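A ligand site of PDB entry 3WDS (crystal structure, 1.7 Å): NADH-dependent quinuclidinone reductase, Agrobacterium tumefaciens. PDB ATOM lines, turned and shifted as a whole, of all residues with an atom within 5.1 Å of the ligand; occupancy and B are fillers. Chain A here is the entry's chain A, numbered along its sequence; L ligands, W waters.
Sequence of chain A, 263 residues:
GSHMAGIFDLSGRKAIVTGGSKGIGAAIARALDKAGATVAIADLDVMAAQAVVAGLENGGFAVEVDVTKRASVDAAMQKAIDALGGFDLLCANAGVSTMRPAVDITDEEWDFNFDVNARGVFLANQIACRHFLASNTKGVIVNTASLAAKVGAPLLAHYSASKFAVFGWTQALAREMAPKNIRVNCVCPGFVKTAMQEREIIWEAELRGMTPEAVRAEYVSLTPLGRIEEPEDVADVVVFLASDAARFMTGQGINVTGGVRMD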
ATOM      1  N   GLY A  19      16.875   1.068  27.348  1.00  0.00           N
ATOM      2  CA  GLY A  19      18.205   1.564  27.220  1.00  0.00           C
ATOM      3  C   GLY A  19      18.887   1.911  28.506  1.00  0.00           C
ATOM      4  O   GLY A  19      19.721   2.840  28.569  1.00  0.00           O
ATOM      5  N   GLY A  20      18.470   1.232  29.560  1.00  0.00           N
ATOM      6  CA  GLY A  20      18.924   1.545  30.905  1.00  0.00           C
ATOM      7  C   GLY A  20      20.189   0.842  31.326  1.00  0.00           C
ATOM      8  O   GLY A  20      20.573   0.982  32.480  1.00  0.00           O
ATOM      9  N   SER A  21      20.844   0.091  30.438  1.00  0.00           N
ATOM     10  CA  SER A  21      22.019  -0.666  30.865  1.00  0.00           C
ATOM     11  C   SER A  21      23.260   0.099  31.208  1.00  0.00           C
ATOM     12  O   SER A  21      24.083  -0.387  31.926  1.00  0.00           O
ATOM     13  CB  SER A  21      22.406  -1.644  29.742  1.00  0.00           C
ATOM     14  OG  SER A  21      21.533  -2.764  29.848  1.00  0.00           O
ATOM     15  N   LYS A  22      23.477   1.227  30.547  1.00  0.00           N
ATOM     16  CA  LYS A  22      24.650   1.994  30.759  1.00  0.00           C
ATOM     17  C   LYS A  22      24.381   3.493  30.531  1.00  0.00           C
ATOM     18  O   LYS A  22      23.292   3.918  30.135  1.00  0.00           O
ATOM     19  CB  LYS A  22      25.755   1.512  29.883  1.00  0.00           C
ATOM     20  CG  LYS A  22      25.448   1.536  28.400  1.00  0.00           C
ATOM     21  CD  LYS A  22      26.284   0.515  27.615  1.00  0.00           C
ATOM     22  CE  LYS A  22      25.998  -0.872  28.124  1.00  0.00           C
ATOM     23  NZ  LYS A  22      26.236  -1.906  27.099  1.00  0.00           N
ATOM     24  N   GLY A  23      25.420   4.277  30.727  1.00  0.00           N
ATOM     25  CA  GLY A  23      25.312   5.719  30.444  1.00  0.00           C
ATOM     26  C   GLY A  23      24.165   6.458  31.105  1.00  0.00           C
ATOM     27  O   GLY A  23      23.832   6.298  32.329  1.00  0.00           O
ATOM     28  N   ILE A  24      23.552   7.342  30.311  1.00  0.00           N
ATOM     29  CA  ILE A  24      22.405   8.089  30.838  1.00  0.00           C
ATOM     30  C   ILE A  24      21.259   7.209  31.348  1.00  0.00           C
ATOM     31  O   ILE A  24      20.661   7.433  32.440  1.00  0.00           O
ATOM     32  CB  ILE A  24      21.857   9.080  29.774  1.00  0.00           C
ATOM     33  CG1 ILE A  24      22.955  10.095  29.394  1.00  0.00           C
ATOM     34  CG2 ILE A  24      20.567   9.688  30.309  1.00  0.00           C
ATOM     35  CD1 ILE A  24      22.633  10.977  28.215  1.00  0.00           C
ATOM     36  N   GLY A  25      21.028   6.089  30.650  1.00  0.00           N
ATOM     37  CA  GLY A  25      19.918   5.217  31.027  1.00  0.00           C
ATOM     38  C   GLY A  25      20.106   4.556  32.374  1.00  0.00           C
ATOM     39  O   GLY A  25      19.181   4.452  33.155  1.00  0.00           O
ATOM     40  N   ALA A  42      14.915  -2.478  30.305  1.00  0.00           N
ATOM     41  CA  ALA A  42      14.798  -3.232  29.038  1.00  0.00           C
ATOM     42  C   ALA A  42      15.857  -2.734  28.118  1.00  0.00           C
ATOM     43  O   ALA A  42      15.956  -1.578  27.866  1.00  0.00           O
ATOM     44  CB  ALA A  42      13.425  -2.992  28.425  1.00  0.00           C
ATOM     45  N   ASP A  43      16.803  -3.585  27.719  1.00  0.00           N
ATOM     46  CA  ASP A  43      17.991  -3.196  27.020  1.00  0.00           C
ATOM     47  C   ASP A  43      18.446  -4.273  26.101  1.00  0.00           C
ATOM     48  O   ASP A  43      18.136  -5.436  26.342  1.00  0.00           O
ATOM     49  CB  ASP A  43      19.129  -2.861  28.030  1.00  0.00           C
ATOM     50  CG  ASP A  43      20.179  -1.997  27.441  1.00  0.00           C
ATOM     51  OD1 ASP A  43      21.072  -2.490  26.675  1.00  0.00           O
ATOM     52  OD2 ASP A  43      20.158  -0.728  27.742  1.00  0.00           O
ATOM     53  N   LEU A  44      19.154  -3.908  25.024  1.00  0.00           N
ATOM     54  CA  LEU A  44      19.751  -4.865  24.083  1.00  0.00           C
ATOM     55  C   LEU A  44      20.788  -5.689  24.784  1.00  0.00           C
ATOM     56  O   LEU A  44      20.921  -6.896  24.469  1.00  0.00           O
ATOM     57  CB  LEU A  44      20.390  -4.123  22.920  1.00  0.00           C
ATOM     58  CG  LEU A  44      20.713  -4.960  21.735  1.00  0.00           C
ATOM     59  CD1 LEU A  44      19.428  -5.369  21.029  1.00  0.00           C
ATOM     60  CD2 LEU A  44      21.545  -4.138  20.822  1.00  0.00           C
ATOM     61  N   ASP A  45      21.408  -5.127  25.798  1.00  0.00           N
ATOM     62  CA  ASP A  45      22.470  -5.829  26.604  1.00  0.00           C
ATOM     63  C   ASP A  45      21.857  -6.191  27.954  1.00  0.00           C
ATOM     64  O   ASP A  45      21.838  -5.335  28.886  1.00  0.00           O
ATOM     65  CB  ASP A  45      23.678  -4.925  26.796  1.00  0.00           C
ATOM     66  CG  ASP A  45      24.843  -5.588  27.567  1.00  0.00           C
ATOM     67  OD1 ASP A  45      24.627  -6.586  28.258  1.00  0.00           O
ATOM     68  OD2 ASP A  45      25.901  -4.919  27.592  1.00  0.00           O
ATOM     69  N   VAL A  65      15.566  -6.428  25.188  1.00  0.00           N
ATOM     70  CA  VAL A  65      14.644  -5.774  24.204  1.00  0.00           C
ATOM     71  C   VAL A  65      15.474  -5.282  23.103  1.00  0.00           C
ATOM     72  O   VAL A  65      16.652  -4.877  23.335  1.00  0.00           O
ATOM     73  CB  VAL A  65      13.750  -4.676  24.814  1.00  0.00           C
ATOM     74  CG1 VAL A  65      14.546  -3.414  25.050  1.00  0.00           C
ATOM     75  CG2 VAL A  65      12.554  -4.417  23.910  1.00  0.00           C
ATOM     76  N   ASP A  66      14.919  -5.351  21.890  1.00  0.00           N
ATOM     77  CA  ASP A  66      15.460  -4.588  20.736  1.00  0.00           C
ATOM     78  C   ASP A  66      14.369  -3.582  20.410  1.00  0.00           C
ATOM     79  O   ASP A  66      13.319  -3.943  19.882  1.00  0.00           O
ATOM     80  CB  ASP A  66      15.853  -5.514  19.539  1.00  0.00           C
ATOM     81  CG  ASP A  66      16.390  -4.769  18.379  1.00  0.00           C
ATOM     82  OD1 ASP A  66      16.206  -3.543  18.346  1.00  0.00           O
ATOM     83  OD2 ASP A  66      16.960  -5.400  17.449  1.00  0.00           O
ATOM     84  N   VAL A  67      14.581  -2.298  20.750  1.00  0.00           N
ATOM     85  CA  VAL A  67      13.511  -1.346  20.553  1.00  0.00           C
ATOM     86  C   VAL A  67      13.185  -1.163  19.090  1.00  0.00           C
ATOM     87  O   VAL A  67      12.241  -0.407  18.796  1.00  0.00           O
ATOM     88  CB  VAL A  67      13.822   0.025  21.239  1.00  0.00           C
ATOM     89  CG1 VAL A  67      13.991  -0.159  22.729  1.00  0.00           C
ATOM     90  CG2 VAL A  67      15.072   0.646  20.683  1.00  0.00           C
ATOM     91  N   THR A  68      13.998  -1.627  18.151  1.00  0.00           N
ATOM     92  CA  THR A  68      13.703  -1.426  16.711  1.00  0.00           C
ATOM     93  C   THR A  68      12.595  -2.362  16.217  1.00  0.00           C
ATOM     94  O   THR A  68      12.115  -2.222  15.069  1.00  0.00           O
ATOM     95  CB  THR A  68      14.914  -1.612  15.833  1.00  0.00           C
ATOM     96  OG1 THR A  68      15.396  -2.979  15.834  1.00  0.00           O
ATOM     97  CG2 THR A  68      16.027  -0.743  16.333  1.00  0.00           C
ATOM     98  N   ASN A  93      14.844   5.742  26.752  1.00  0.00           N
ATOM     99  CA  ASN A  93      16.192   6.236  26.613  1.00  0.00           C
ATOM    100  C   ASN A  93      17.076   5.654  25.537  1.00  0.00           C
ATOM    101  O   ASN A  93      18.043   6.330  25.111  1.00  0.00           O
ATOM    102  CB  ASN A  93      16.852   6.189  27.980  1.00  0.00           C
ATOM    103  CG  ASN A  93      18.316   6.539  27.937  1.00  0.00           C
ATOM    104  OD1 ASN A  93      19.237   5.660  27.981  1.00  0.00           O
ATOM    105  ND2 ASN A  93      18.570   7.836  27.979  1.00  0.00           N
ATOM    106  N   ALA A  94      16.803   4.429  25.053  1.00  0.00           N
ATOM    107  CA  ALA A  94      17.727   3.750  24.127  1.00  0.00           C
ATOM    108  C   ALA A  94      17.990   4.676  22.949  1.00  0.00           C
ATOM    109  O   ALA A  94      17.048   5.290  22.372  1.00  0.00           O
ATOM    110  CB  ALA A  94      17.105   2.487  23.632  1.00  0.00           C
ATOM    111  N   GLY A  95      19.244   4.822  22.617  1.00  0.00           N
ATOM    112  CA  GLY A  95      19.647   5.549  21.376  1.00  0.00           C
ATOM    113  C   GLY A  95      21.014   5.190  20.912  1.00  0.00           C
ATOM    114  O   GLY A  95      21.820   4.601  21.704  1.00  0.00           O
ATOM    115  N   VAL A  96      21.291   5.492  19.655  1.00  0.00           N
ATOM    116  CA  VAL A  96      22.545   5.270  19.045  1.00  0.00           C
ATOM    117  C   VAL A  96      22.964   6.517  18.245  1.00  0.00           C
ATOM    118  O   VAL A  96      22.087   7.378  17.937  1.00  0.00           O
ATOM    119  CB  VAL A  96      22.516   4.114  18.080  1.00  0.00           C
ATOM    120  CG1 VAL A  96      22.201   2.811  18.835  1.00  0.00           C
ATOM    121  CG2 VAL A  96      21.504   4.352  16.947  1.00  0.00           C
ATOM    122  N   VAL A 116      16.451   2.986  15.917  1.00  0.00           N
ATOM    123  CA  VAL A 116      16.577   3.046  17.347  1.00  0.00           C
ATOM    124  C   VAL A 116      15.949   4.282  17.949  1.00  0.00           C
ATOM    125  O   VAL A 116      15.127   4.233  18.928  1.00  0.00           O
ATOM    126  CB  VAL A 116      18.072   2.891  17.786  1.00  0.00           C
ATOM    127  CG1 VAL A 116      18.136   2.863  19.273  1.00  0.00           C
ATOM    128  CG2 VAL A 116      18.654   1.574  17.241  1.00  0.00           C
ATOM    129  N   ASN A 117      16.420   5.430  17.439  1.00  0.00           N
ATOM    130  CA  ASN A 117      16.175   6.661  18.131  1.00  0.00           C
ATOM    131  C   ASN A 117      14.731   7.069  17.989  1.00  0.00           C
ATOM    132  O   ASN A 117      14.138   7.524  18.954  1.00  0.00           O
ATOM    133  CB  ASN A 117      17.064   7.789  17.623  1.00  0.00           C
ATOM    134  CG  ASN A 117      18.517   7.542  17.863  1.00  0.00           C
ATOM    135  OD1 ASN A 117      18.885   6.675  18.699  1.00  0.00           O
ATOM    136  ND2 ASN A 117      19.362   8.230  17.137  1.00  0.00           N
ATOM    137  N   THR A 144      14.284  10.393  26.061  1.00  0.00           N
ATOM    138  CA  THR A 144      15.584  11.029  25.918  1.00  0.00           C
ATOM    139  C   THR A 144      15.830  11.480  24.475  1.00  0.00           C
ATOM    140  O   THR A 144      15.978  10.661  23.563  1.00  0.00           O
ATOM    141  CB  THR A 144      16.753  10.140  26.323  1.00  0.00           C
ATOM    142  OG1 THR A 144      16.493   9.627  27.626  1.00  0.00           O
ATOM    143  CG2 THR A 144      17.966  10.979  26.402  1.00  0.00           C
ATOM    144  N   ALA A 145      15.720  12.799  24.248  1.00  0.00           N
ATOM    145  CA  ALA A 145      16.025  13.382  22.923  1.00  0.00           C
ATOM    146  C   ALA A 145      17.507  13.766  22.896  1.00  0.00           C
ATOM    147  O   ALA A 145      18.402  12.922  23.206  1.00  0.00           O
ATOM    148  CB  ALA A 145      15.050  14.518  22.643  1.00  0.00           C
ATOM    149  N   SER A 146      17.811  15.028  22.652  1.00  0.00           N
ATOM    150  CA  SER A 146      19.209  15.452  22.525  1.00  0.00           C
ATOM    151  C   SER A 146      19.169  16.961  22.320  1.00  0.00           C
ATOM    152  O   SER A 146      18.152  17.490  21.803  1.00  0.00           O
ATOM    153  CB  SER A 146      19.802  14.850  21.297  1.00  0.00           C
ATOM    154  OG  SER A 146      21.151  15.203  21.018  1.00  0.00           O
ATOM    155  N   LEU A 147      20.331  17.581  22.567  1.00  0.00           N
ATOM    156  CA  LEU A 147      20.614  18.936  22.101  1.00  0.00           C
ATOM    157  C   LEU A 147      20.341  18.951  20.616  1.00  0.00           C
ATOM    158  O   LEU A 147      19.862  19.980  20.053  1.00  0.00           O
ATOM    159  CB  LEU A 147      22.066  19.339  22.397  1.00  0.00           C
ATOM    160  CG  LEU A 147      22.697  20.572  21.751  1.00  0.00           C
ATOM    161  CD1 LEU A 147      21.870  21.734  22.196  1.00  0.00           C
ATOM    162  CD2 LEU A 147      24.147  20.640  22.236  1.00  0.00           C
ATOM    163  N   TYR A 159      21.467  11.813  12.667  1.00  0.00           N
ATOM    164  CA  TYR A 159      21.206  11.703  14.093  1.00  0.00           C
ATOM    165  C   TYR A 159      20.293  12.837  14.597  1.00  0.00           C
ATOM    166  O   TYR A 159      19.259  12.566  15.234  1.00  0.00           O
ATOM    167  CB  TYR A 159      22.513  11.685  14.847  1.00  0.00           C
ATOM    168  CG  TYR A 159      22.351  11.763  16.387  1.00  0.00           C
ATOM    169  CD1 TYR A 159      22.147  10.608  17.090  1.00  0.00           C
ATOM    170  CD2 TYR A 159      22.472  12.934  17.077  1.00  0.00           C
ATOM    171  CE1 TYR A 159      22.011  10.630  18.508  1.00  0.00           C
ATOM    172  CE2 TYR A 159      22.364  12.961  18.454  1.00  0.00           C
ATOM    173  CZ  TYR A 159      22.154  11.819  19.154  1.00  0.00           C
ATOM    174  OH  TYR A 159      21.971  11.862  20.543  1.00  0.00           O
ATOM    175  N   LYS A 163      16.502  12.753  16.129  1.00  0.00           N
ATOM    176  CA  LYS A 163      16.212  13.329  17.438  1.00  0.00           C
ATOM    177  C   LYS A 163      15.174  14.450  17.369  1.00  0.00           C
ATOM    178  O   LYS A 163      14.320  14.539  18.234  1.00  0.00           O
ATOM    179  CB  LYS A 163      17.518  13.733  18.109  1.00  0.00           C
ATOM    180  CG  LYS A 163      18.356  12.537  18.567  1.00  0.00           C
ATOM    181  CD  LYS A 163      17.705  11.777  19.696  1.00  0.00           C
ATOM    182  CE  LYS A 163      18.729  10.789  20.344  1.00  0.00           C
ATOM    183  NZ  LYS A 163      18.022  10.164  21.499  1.00  0.00           N
ATOM    184  N   PRO A 189      19.724  16.420  26.424  1.00  0.00           N
ATOM    185  CA  PRO A 189      21.035  16.560  27.041  1.00  0.00           C
ATOM    186  C   PRO A 189      22.060  17.210  26.142  1.00  0.00           C
ATOM    187  O   PRO A 189      21.943  17.102  24.906  1.00  0.00           O
ATOM    188  CB  PRO A 189      21.472  15.101  27.352  1.00  0.00           C
ATOM    189  CG  PRO A 189      20.267  14.293  27.162  1.00  0.00           C
ATOM    190  CD  PRO A 189      19.336  15.030  26.230  1.00  0.00           C
ATOM    191  N   GLY A 190      23.094  17.775  26.757  1.00  0.00           N
ATOM    192  CA  GLY A 190      24.196  18.406  26.041  1.00  0.00           C
ATOM    193  C   GLY A 190      25.338  17.409  25.892  1.00  0.00           C
ATOM    194  O   GLY A 190      25.106  16.279  25.448  1.00  0.00           O
ATOM    195  N   PHE A 191      26.548  17.811  26.291  1.00  0.00           N
ATOM    196  CA  PHE A 191      27.741  17.044  25.938  1.00  0.00           C
ATOM    197  C   PHE A 191      28.048  16.110  27.125  1.00  0.00           C
ATOM    198  O   PHE A 191      28.849  16.417  28.012  1.00  0.00           O
ATOM    199  CB  PHE A 191      28.848  18.093  25.690  1.00  0.00           C
ATOM    200  CG  PHE A 191      28.583  19.053  24.595  1.00  0.00           C
ATOM    201  CD1 PHE A 191      28.366  18.588  23.308  1.00  0.00           C
ATOM    202  CD2 PHE A 191      28.620  20.441  24.805  1.00  0.00           C
ATOM    203  CE1 PHE A 191      28.140  19.507  22.283  1.00  0.00           C
ATOM    204  CE2 PHE A 191      28.378  21.326  23.801  1.00  0.00           C
ATOM    205  CZ  PHE A 191      28.129  20.865  22.529  1.00  0.00           C
ATOM    206  N   VAL A 192      27.395  14.960  27.182  1.00  0.00           N
ATOM    207  CA  VAL A 192      27.471  14.092  28.342  1.00  0.00           C
ATOM    208  C   VAL A 192      28.557  13.037  28.221  1.00  0.00           C
ATOM    209  O   VAL A 192      28.642  12.284  27.213  1.00  0.00           O
ATOM    210  CB  VAL A 192      26.140  13.311  28.532  1.00  0.00           C
ATOM    211  CG1 VAL A 192      26.109  12.496  29.820  1.00  0.00           C
ATOM    212  CG2 VAL A 192      24.946  14.255  28.468  1.00  0.00           C
ATOM    213  N   THR A 194      29.978   9.829  28.486  1.00  0.00           N
ATOM    214  CA  THR A 194      29.626   8.399  28.507  1.00  0.00           C
ATOM    215  C   THR A 194      30.439   7.731  27.385  1.00  0.00           C
ATOM    216  O   THR A 194      31.273   8.351  26.789  1.00  0.00           O
ATOM    217  CB  THR A 194      28.222   8.193  28.013  1.00  0.00           C
ATOM    218  OG1 THR A 194      28.155   8.539  26.612  1.00  0.00           O
ATOM    219  CG2 THR A 194      27.211   9.003  28.787  1.00  0.00           C
ATOM    220  N   ALA A 195      30.166   6.443  27.039  1.00  0.00           N
ATOM    221  CA  ALA A 195      30.900   5.824  25.894  1.00  0.00           C
ATOM    222  C   ALA A 195      30.487   6.435  24.509  1.00  0.00           C
ATOM    223  O   ALA A 195      31.309   6.564  23.588  1.00  0.00           O
ATOM    224  CB  ALA A 195      30.660   4.337  25.898  1.00  0.00           C
ATOM    225  N   MET A 196      29.235   6.866  24.379  1.00  0.00           N
ATOM    226  CA  MET A 196      28.854   7.664  23.173  1.00  0.00           C
ATOM    227  C   MET A 196      29.774   8.870  22.952  1.00  0.00           C
ATOM    228  O   MET A 196      30.184   9.166  21.820  1.00  0.00           O
ATOM    229  CB  MET A 196      27.396   8.116  23.185  1.00  0.00           C
ATOM    230  CG  MET A 196      27.038   8.841  21.913  1.00  0.00           C
ATOM    231  SD  MET A 196      25.232   9.135  21.706  1.00  0.00           S
ATOM    232  CE  MET A 196      24.591   7.448  21.607  1.00  0.00           C
ATOM    233  N   GLN A 197      30.104   9.555  24.051  1.00  0.00           N
ATOM    234  CA  GLN A 197      30.982  10.662  23.947  1.00  0.00           C
ATOM    235  C   GLN A 197      32.416  10.187  23.636  1.00  0.00           C
ATOM    236  O   GLN A 197      33.061  10.791  22.788  1.00  0.00           O
ATOM    237  CB  GLN A 197      30.952  11.536  25.190  1.00  0.00           C
ATOM    238  CG  GLN A 197      31.866  12.717  25.022  1.00  0.00           C
ATOM    239  CD  GLN A 197      31.896  13.651  26.192  1.00  0.00           C
ATOM    240  OE1 GLN A 197      32.898  13.718  26.991  1.00  0.00           O
ATOM    241  NE2 GLN A 197      30.860  14.456  26.280  1.00  0.00           N
ATOM    242  N   ARG A 199      33.512   7.692  22.066  1.00  0.00           N
ATOM    243  CA  ARG A 199      33.495   7.322  20.647  1.00  0.00           C
ATOM    244  C   ARG A 199      33.478   8.481  19.758  1.00  0.00           C
ATOM    245  O   ARG A 199      34.233   8.529  18.806  1.00  0.00           O
ATOM    246  CB  ARG A 199      32.233   6.502  20.258  1.00  0.00           C
ATOM    247  CG  ARG A 199      32.161   5.106  20.863  1.00  0.00           C
ATOM    248  CD  ARG A 199      31.052   4.288  20.189  1.00  0.00           C
ATOM    249  NE  ARG A 199      29.680   4.712  20.548  1.00  0.00           N
ATOM    250  CZ  ARG A 199      29.011   4.267  21.606  1.00  0.00           C
ATOM    251  NH1 ARG A 199      27.760   4.690  21.829  1.00  0.00           N
ATOM    252  NH2 ARG A 199      29.587   3.399  22.450  1.00  0.00           N
ATOM    253  N   GLU A 200      32.546   9.378  20.025  1.00  0.00           N
ATOM    254  CA  GLU A 200      32.280  10.518  19.159  1.00  0.00           C
ATOM    255  C   GLU A 200      33.501  11.407  19.139  1.00  0.00           C
ATOM    256  O   GLU A 200      33.791  11.972  18.106  1.00  0.00           O
ATOM    257  CB  GLU A 200      31.030  11.306  19.597  1.00  0.00           C
ATOM    258  CG  GLU A 200      29.705  10.745  18.967  1.00  0.00           C
ATOM    259  CD  GLU A 200      28.419  11.414  19.439  1.00  0.00           C
ATOM    260  OE1 GLU A 200      27.315  10.942  19.043  1.00  0.00           O
ATOM    261  OE2 GLU A 200      28.466  12.437  20.182  1.00  0.00           O
HETATM  262  P1  LIG L   1      25.277   4.668  25.438  1.00  0.00           P
HETATM  263  O1  LIG L   1      25.785   4.369  24.057  1.00  0.00           O
HETATM  264  O2  LIG L   1      26.210   4.779  26.621  1.00  0.00           O
HETATM  265  O3  LIG L   1      24.011   3.772  25.888  1.00  0.00           O
HETATM  266  C1  LIG L   1      23.044   3.375  24.902  1.00  0.00           C
HETATM  267  C2  LIG L   1      22.125   2.426  25.666  1.00  0.00           C
HETATM  268  O4  LIG L   1      21.035   2.132  24.766  1.00  0.00           O
HETATM  269  C3  LIG L   1      22.867   1.106  26.007  1.00  0.00           C
HETATM  270  O5  LIG L   1      22.397   0.550  27.272  1.00  0.00           O
HETATM  271  C4  LIG L   1      22.454   0.213  24.813  1.00  0.00           C
HETATM  272  O6  LIG L   1      22.534  -1.231  24.980  1.00  0.00           O
HETATM  273  C5  LIG L   1      21.042   0.710  24.522  1.00  0.00           C
HETATM  274  N1  LIG L   1      20.588   0.325  23.168  1.00  0.00           N
HETATM  275  C6  LIG L   1      21.238   0.585  21.990  1.00  0.00           C
HETATM  276  N2  LIG L   1      20.503   0.087  20.965  1.00  0.00           N
HETATM  277  C7  LIG L   1      19.382  -0.528  21.500  1.00  0.00           C
HETATM  278  C8  LIG L   1      18.244  -1.341  20.978  1.00  0.00           C
HETATM  279  N3  LIG L   1      18.149  -1.482  19.583  1.00  0.00           N
HETATM  280  N4  LIG L   1      17.296  -1.801  21.929  1.00  0.00           N
HETATM  281  C9  LIG L   1      17.444  -1.554  23.252  1.00  0.00           C
HETATM  282  N5  LIG L   1      18.539  -0.902  23.811  1.00  0.00           N
HETATM  283  C10 LIG L   1      19.467  -0.357  22.953  1.00  0.00           C
HETATM  284  O7  LIG L   1      24.822   6.156  25.118  1.00  0.00           O
HETATM  285  P2  LIG L   1      24.486   7.415  26.116  1.00  0.00           P
HETATM  286  O8  LIG L   1      25.535   8.489  25.796  1.00  0.00           O
HETATM  287  O9  LIG L   1      24.123   7.078  27.566  1.00  0.00           O
HETATM  288  O10 LIG L   1      23.079   7.898  25.364  1.00  0.00           O
HETATM  289  C11 LIG L   1      21.777   7.545  25.930  1.00  0.00           C
HETATM  290  C12 LIG L   1      20.687   8.379  25.280  1.00  0.00           C
HETATM  291  O11 LIG L   1      21.114   9.762  25.426  1.00  0.00           O
HETATM  292  C13 LIG L   1      20.577   8.116  23.762  1.00  0.00           C
HETATM  293  O12 LIG L   1      19.219   8.363  23.330  1.00  0.00           O
HETATM  294  C14 LIG L   1      21.535   9.134  23.166  1.00  0.00           C
HETATM  295  O13 LIG L   1      21.211   9.531  21.852  1.00  0.00           O
HETATM  296  C15 LIG L   1      21.273  10.279  24.127  1.00  0.00           C
HETATM  297  N6  LIG L   1      22.270  11.313  24.204  1.00  0.00           N
HETATM  298  C16 LIG L   1      23.562  11.102  24.607  1.00  0.00           C
HETATM  299  C17 LIG L   1      24.379  12.229  24.634  1.00  0.00           C
HETATM  300  C18 LIG L   1      25.858  12.209  24.993  1.00  0.00           C
HETATM  301  O14 LIG L   1      26.379  11.162  25.437  1.00  0.00           O
HETATM  302  N7  LIG L   1      26.530  13.379  24.781  1.00  0.00           N
HETATM  303  C19 LIG L   1      23.822  13.471  24.324  1.00  0.00           C
HETATM  304  C20 LIG L   1      22.536  13.641  23.944  1.00  0.00           C
HETATM  305  C21 LIG L   1      21.770  12.527  23.904  1.00  0.00           C
HETATM  306  O   HOH W   1      25.832  15.170  22.485  1.00  0.00           O
HETATM  307  O   HOH W   2      24.434   3.861  21.676  1.00  0.00           O
HETATM  308  O   HOH W   3      24.035  -3.076  23.621  1.00  0.00           O
HETATM  309  O   HOH W   4      29.033  14.377  24.055  1.00  0.00           O
HETATM  310  O   HOH W   5      21.635  -0.738  18.618  1.00  0.00           O
HETATM  311  O   HOH W   6      22.029   5.359  28.056  1.00  0.00           O
HETATM  312  O   HOH W   7      28.134   4.593  28.102  1.00  0.00           O
HETATM  313  O   HOH W   8      24.527   1.086  21.833  1.00  0.00           O
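O1 of the ligand lies within salt-bridge range of NH1 of Arg 199. O of Gly 190 sits close to N7 of the ligand, 3.3 Å away. An oxygen (O8) of the ligand lies within hydrogen-bond range of the side-chain hydroxyl of Thr 194. The backbone carbonyl oxygen (O) of Val 192 sits at hydrogen-bond distance from a nitrogen (N7) of the ligand (3.4 Å). A nitrogen (N5) of the ligand sits at hydrogen-bond distance from the backbone NH (N) of Leu 44. OD1 of Asp 43 is in hydrogen-bond range of O6 of the ligand. A nitrogen (N3) of the ligand is in hydrogen-bond range of the side-chain carboxylate (OD1) of Asp 66 (3.1 Å). N of Val 67 is in hydrogen-bond range of N4 of the ligand, at 3.0 Å. O12 of the ligand is in hydrogen-bond range of O of Asn 93 (2.9 Å). The side-chain amino group (NZ) of Lys 163 sits at hydrogen-bond distance from an oxygen (O12) of the ligand. OH of Tyr 159 lies within hydrogen-bond range of O13 of the ligand (2.8 Å). The backbone NH (N) of Ile 24 is in hydrogen-bond range of an oxygen (O9) of the ligand.
Water W7 bridges O2 of the ligand (2.4 Å) and N of Ala 195 (2.9 Å). Water W2 lies within hydrogen-bond range of the backbone carbonyl oxygen of Gly 95 (2.7 Å), an oxygen (O1) of the ligand (2.8 Å) and the guanidinium group of Arg 199 (3.4 Å). Water W4 bridges N7 of the ligand (2.8 Å) and NE2 of Gln 197 (2.9 Å). Water W1 bridges a nitrogen (N7) of the ligand (3.0 Å) and the backbone carbonyl oxygen (O) of Gly 190 (3.2 Å).
The side-chain amide oxygen (OD1) of Asn 93 lies close to the backbone NH (N) of Gly 25 (3.2 Å). The side-chain carboxylate (OD2) of Asp 45 is in salt-bridge range of the side-chain amino group (NZ) of Lys 22. NE2 of Gln 197 lies close to O of Val 192 (3.2 Å). The side-chain carboxylate (OD2) of Asp 43 lies within hydrogen-bond range of the backbone NH (N) of Gly 20, at 3.2 Å. The side-chain amino group (NZ) of Lys 163 lies within hydrogen-bond range of the backbone carbonyl oxygen (O) of Thr 144 (2.9 Å). The backbone NH of Gln 197 lies within hydrogen-bond range of the side-chain hydroxyl of Thr 194 (3.4 Å). The side-chain carboxylate (OD2) of Asp 43 lies within hydrogen-bond range of the backbone NH (N) of Ser 21, at 2.9 Å. N of Asp 45 sits at hydrogen-bond distance from OD1 of Asp 43 (2.8 Å).
The backbone carbonyl oxygen of Val 65 lies close to a nitrogen (N4) of the ligand. Gly 19 touches the ligand. Ser 21 touches the ligand (CB to O5, 3.3 Å). Lys 22 touches the ligand (CG to O5, 3.4 Å). CA of Gly 23 touches O9 of the ligand, 3.4 Å away. Thr 68 touches the ligand. Ala 94 touches the ligand. CA of Gly 95 touches O12 of the ligand, 3.5 Å away. Val 96 touches the ligand (CG1 to N2, 3.9 Å). Val 116 touches the ligand. CG2 of Thr 144 touches O11 of the ligand, at 3.5 Å. Ala 145 touches the ligand (O to C21, 3.5 Å). Ser 146 touches the ligand. O of Pro 189 touches C20 of the ligand, 3.6 Å away. Phe 191 touches the ligand. Met 196 touches the ligand (CB to O8, 3.2 Å). Hydrophobic or aromatic side chains within 4 Å of the ligand: Ile 24, Leu 44, Val 65, Val 67, Ala 94, Val 96, Val 116, Tyr 159, Pro 189, Val 192 and Met 196. Of the 37 residues printed, 28 come within 4 Å of the ligand. Along chain A the residues within 4 Å of the ligand span positions 19 to 199.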
